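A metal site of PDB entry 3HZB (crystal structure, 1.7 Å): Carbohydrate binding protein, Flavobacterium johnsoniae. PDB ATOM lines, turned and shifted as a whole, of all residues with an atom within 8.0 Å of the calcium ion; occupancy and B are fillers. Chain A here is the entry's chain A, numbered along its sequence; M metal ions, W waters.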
ATOM      1  N   TYR A   6      15.246  31.740  -4.589  1.00  0.00           N
ATOM      2  CA  TYR A   6      15.220  32.077  -3.172  1.00  0.00           C
ATOM      3  C   TYR A   6      15.244  30.891  -2.233  1.00  0.00           C
ATOM      4  O   TYR A   6      14.691  29.822  -2.527  1.00  0.00           O
ATOM      5  CB  TYR A   6      13.969  32.893  -2.854  1.00  0.00           C
ATOM      6  CG  TYR A   6      13.813  34.143  -3.680  1.00  0.00           C
ATOM      7  CD1 TYR A   6      13.351  34.081  -5.001  1.00  0.00           C
ATOM      8  CD2 TYR A   6      14.090  35.399  -3.146  1.00  0.00           C
ATOM      9  CE1 TYR A   6      13.181  35.237  -5.758  1.00  0.00           C
ATOM     10  CE2 TYR A   6      13.926  36.558  -3.891  1.00  0.00           C
ATOM     11  CZ  TYR A   6      13.466  36.476  -5.192  1.00  0.00           C
ATOM     12  OH  TYR A   6      13.306  37.619  -5.934  1.00  0.00           O
ATOM     13  N   LYS A   7      15.864  31.110  -1.078  1.00  0.00           N
ATOM     14  CA  LYS A   7      15.973  30.081  -0.063  1.00  0.00           C
ATOM     15  C   LYS A   7      14.616  29.710   0.485  1.00  0.00           C
ATOM     16  O   LYS A   7      14.314  28.538   0.647  1.00  0.00           O
ATOM     17  CB  LYS A   7      16.860  30.558   1.092  1.00  0.00           C
ATOM     18  CG  LYS A   7      17.142  29.483   2.137  1.00  0.00           C
ATOM     19  CD  LYS A   7      17.924  30.052   3.319  1.00  0.00           C
ATOM     20  CE  LYS A   7      18.460  28.945   4.214  1.00  0.00           C
ATOM     21  NZ  LYS A   7      19.523  28.144   3.533  1.00  0.00           N
ATOM     22  N   ASP A   8      13.763  30.690   0.760  1.00  0.00           N
ATOM     23  CA  ASP A   8      12.454  30.380   1.313  1.00  0.00           C
ATOM     24  C   ASP A   8      11.304  30.611   0.347  1.00  0.00           C
ATOM     25  O   ASP A   8      11.481  31.193  -0.718  1.00  0.00           O
ATOM     26  CB  ASP A   8      12.222  31.190   2.591  1.00  0.00           C
ATOM     27  CG  ASP A   8      13.340  31.024   3.597  1.00  0.00           C
ATOM     28  OD1 ASP A   8      13.719  29.857   3.869  1.00  0.00           O
ATOM     29  OD2 ASP A   8      13.828  32.049   4.120  1.00  0.00           O
ATOM     30  N   CYS A   9      10.119  30.142   0.730  1.00  0.00           N
ATOM     31  CA  CYS A   9       8.945  30.311  -0.103  1.00  0.00           C
ATOM     32  C   CYS A   9       8.528  31.785  -0.118  1.00  0.00           C
ATOM     33  O   CYS A   9       8.950  32.554   0.742  1.00  0.00           O
ATOM     34  CB  CYS A   9       7.814  29.406   0.408  1.00  0.00           C
ATOM     35  SG  CYS A   9       8.055  27.691  -0.170  1.00  0.00           S
ATOM     36  N   THR A  12      11.506  35.003  -0.505  1.00  0.00           N
ATOM     37  CA  THR A  12      12.190  35.565   0.643  1.00  0.00           C
ATOM     38  C   THR A  12      13.405  34.690   0.979  1.00  0.00           C
ATOM     39  O   THR A  12      13.522  33.577   0.462  1.00  0.00           O
ATOM     40  CB  THR A  12      11.268  35.652   1.875  1.00  0.00           C
ATOM     41  OG1 THR A  12      10.818  34.332   2.213  1.00  0.00           O
ATOM     42  CG2 THR A  12      10.056  36.526   1.570  1.00  0.00           C
ATOM     43  N   ASN A  35      22.760  23.752  -2.068  1.00  0.00           N
ATOM     44  CA  ASN A  35      22.168  22.546  -2.637  1.00  0.00           C
ATOM     45  C   ASN A  35      20.928  22.198  -1.820  1.00  0.00           C
ATOM     46  O   ASN A  35      20.879  22.525  -0.632  1.00  0.00           O
ATOM     47  CB  ASN A  35      23.171  21.393  -2.533  1.00  0.00           C
ATOM     48  CG  ASN A  35      22.649  20.110  -3.130  1.00  0.00           C
ATOM     49  OD1 ASN A  35      22.511  19.099  -2.434  1.00  0.00           O
ATOM     50  ND2 ASN A  35      22.364  20.143  -4.421  1.00  0.00           N
ATOM     51  N   ASP A  36      19.955  21.537  -2.440  1.00  0.00           N
ATOM     52  CA  ASP A  36      18.730  21.127  -1.759  1.00  0.00           C
ATOM     53  C   ASP A  36      18.279  22.216  -0.803  1.00  0.00           C
ATOM     54  O   ASP A  36      18.077  21.970   0.383  1.00  0.00           O
ATOM     55  CB  ASP A  36      18.983  19.838  -0.956  1.00  0.00           C
ATOM     56  CG  ASP A  36      19.269  18.648  -1.858  1.00  0.00           C
ATOM     57  OD1 ASP A  36      19.214  18.830  -3.092  1.00  0.00           O
ATOM     58  OD2 ASP A  36      19.532  17.548  -1.341  1.00  0.00           O
ATOM     59  N   ASP A  37      18.086  23.416  -1.341  1.00  0.00           N
ATOM     60  CA  ASP A  37      17.724  24.540  -0.495  1.00  0.00           C
ATOM     61  C   ASP A  37      16.737  25.526  -1.124  1.00  0.00           C
ATOM     62  O   ASP A  37      16.034  26.222  -0.409  1.00  0.00           O
ATOM     63  CB  ASP A  37      19.021  25.266  -0.128  1.00  0.00           C
ATOM     64  CG  ASP A  37      18.833  26.255   1.002  1.00  0.00           C
ATOM     65  OD1 ASP A  37      19.185  27.433   0.798  1.00  0.00           O
ATOM     66  OD2 ASP A  37      18.353  25.844   2.081  1.00  0.00           O
ATOM     67  N   ILE A  38      16.687  25.609  -2.449  1.00  0.00           N
ATOM     68  CA  ILE A  38      15.781  26.549  -3.086  1.00  0.00           C
ATOM     69  C   ILE A  38      14.321  26.185  -2.860  1.00  0.00           C
ATOM     70  O   ILE A  38      13.956  25.012  -2.922  1.00  0.00           O
ATOM     71  CB  ILE A  38      16.061  26.624  -4.608  1.00  0.00           C
ATOM     72  CG1 ILE A  38      17.470  27.192  -4.832  1.00  0.00           C
ATOM     73  CG2 ILE A  38      15.006  27.491  -5.298  1.00  0.00           C
ATOM     74  CD1 ILE A  38      17.980  27.002  -6.241  1.00  0.00           C
ATOM     75  N   SER A  39      13.491  27.189  -2.583  1.00  0.00           N
ATOM     76  CA  SER A  39      12.073  26.954  -2.344  1.00  0.00           C
ATOM     77  C   SER A  39      11.118  27.753  -3.228  1.00  0.00           C
ATOM     78  O   SER A  39       9.932  27.430  -3.324  1.00  0.00           O
ATOM     79  CB  SER A  39      11.731  27.227  -0.885  1.00  0.00           C
ATOM     80  OG  SER A  39      12.209  26.152  -0.101  1.00  0.00           O
ATOM     81  N   SER A  40      11.610  28.816  -3.851  1.00  0.00           N
ATOM     82  CA  SER A  40      10.784  29.621  -4.758  1.00  0.00           C
ATOM     83  C   SER A  40      11.687  30.322  -5.746  1.00  0.00           C
ATOM     84  O   SER A  40      12.898  30.439  -5.519  1.00  0.00           O
ATOM     85  CB  SER A  40       9.936  30.634  -3.984  1.00  0.00           C
ATOM     86  OG  SER A  40      10.732  31.615  -3.349  1.00  0.00           O
ATOM     87  N   LEU A  71       7.830  25.668  -4.208  1.00  0.00           N
ATOM     88  CA  LEU A  71       7.953  24.407  -4.927  1.00  0.00           C
ATOM     89  C   LEU A  71       7.256  23.285  -4.162  1.00  0.00           C
ATOM     90  O   LEU A  71       7.174  23.321  -2.931  1.00  0.00           O
ATOM     91  CB  LEU A  71       9.432  24.077  -5.130  1.00  0.00           C
ATOM     92  CG  LEU A  71      10.187  25.049  -6.044  1.00  0.00           C
ATOM     93  CD1 LEU A  71      11.700  24.806  -5.942  1.00  0.00           C
ATOM     94  CD2 LEU A  71       9.708  24.878  -7.484  1.00  0.00           C
ATOM     95  N   ASN A  76      10.873  21.023  -3.676  1.00  0.00           N
ATOM     96  CA  ASN A  76      11.326  21.920  -2.621  1.00  0.00           C
ATOM     97  C   ASN A  76      12.533  21.359  -1.896  1.00  0.00           C
ATOM     98  O   ASN A  76      12.539  20.202  -1.490  1.00  0.00           O
ATOM     99  CB  ASN A  76      10.203  22.169  -1.610  1.00  0.00           C
ATOM    100  CG  ASN A  76      10.618  23.124  -0.510  1.00  0.00           C
ATOM    101  OD1 ASN A  76      11.025  24.244  -0.780  1.00  0.00           O
ATOM    102  ND2 ASN A  76      10.541  22.673   0.733  1.00  0.00           N
ATOM    103  N   ASP A  77      13.572  22.186  -1.744  1.00  0.00           N
ATOM    104  CA  ASP A  77      14.807  21.767  -1.081  1.00  0.00           C
ATOM    105  C   ASP A  77      15.429  20.536  -1.719  1.00  0.00           C
ATOM    106  O   ASP A  77      15.981  19.688  -1.030  1.00  0.00           O
ATOM    107  CB  ASP A  77      14.549  21.480   0.404  1.00  0.00           C
ATOM    108  CG  ASP A  77      14.140  22.709   1.162  1.00  0.00           C
ATOM    109  OD1 ASP A  77      14.444  23.796   0.651  1.00  0.00           O
ATOM    110  OD2 ASP A  77      13.536  22.593   2.244  1.00  0.00           O
ATOM    111  N   LYS A  78      15.314  20.433  -3.041  1.00  0.00           N
ATOM    112  CA  LYS A  78      15.859  19.283  -3.759  1.00  0.00           C
ATOM    113  C   LYS A  78      16.688  19.649  -4.994  1.00  0.00           C
ATOM    114  O   LYS A  78      17.386  18.805  -5.545  1.00  0.00           O
ATOM    115  CB  LYS A  78      14.717  18.367  -4.198  1.00  0.00           C
ATOM    116  CG  LYS A  78      13.965  17.707  -3.059  1.00  0.00           C
ATOM    117  CD  LYS A  78      14.839  16.702  -2.331  1.00  0.00           C
ATOM    118  CE  LYS A  78      14.086  16.022  -1.202  1.00  0.00           C
ATOM    119  NZ  LYS A  78      14.978  15.078  -0.466  1.00  0.00           N
HETATM  120 CA    CA M   1      14.255  26.203   1.335  1.00  0.00          CA
HETATM  121  O   HOH W   1      16.083  25.865   3.097  1.00  0.00           O
HETATM  122  O   HOH W   2      12.482  24.903   2.884  1.00  0.00           O
HETATM  123  O   HOH W   3      12.907  27.383   3.543  1.00  0.00           O
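Within 4 Å of the calcium ion: Lys 7, Asp 37, Ser 39 and Asp 77.
The calcium ion is bound by the backbone carbonyl oxygen of Lys 7 (2.4 Å), the backbone carbonyl oxygen of Asp 37 (2.5 Å), the side-chain hydroxyl of Ser 39 (2.5 Å), the side-chain carboxylate of Asp 77 (2.5 Å), water W1 (2.6 Å), water W2 (2.7 Å) and water W3 (2.8 Å).
The backbone NH (N) of Ser 39 sits at hydrogen-bond distance from the backbone carbonyl oxygen (O) of Tyr 6 (2.9 Å). The backbone carbonyl oxygen (O) of Ser 39 lies within hydrogen-bond range of the backbone NH (N) of Leu 71 (2.9 Å). The backbone carbonyl oxygen of Ile 38 sits at hydrogen-bond distance from the backbone NH of Asp 77, at 3.1 Å. The side-chain carboxylate of Asp 77 sits at hydrogen-bond distance from the side-chain amide nitrogen of Asn 76 (3.4 Å).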
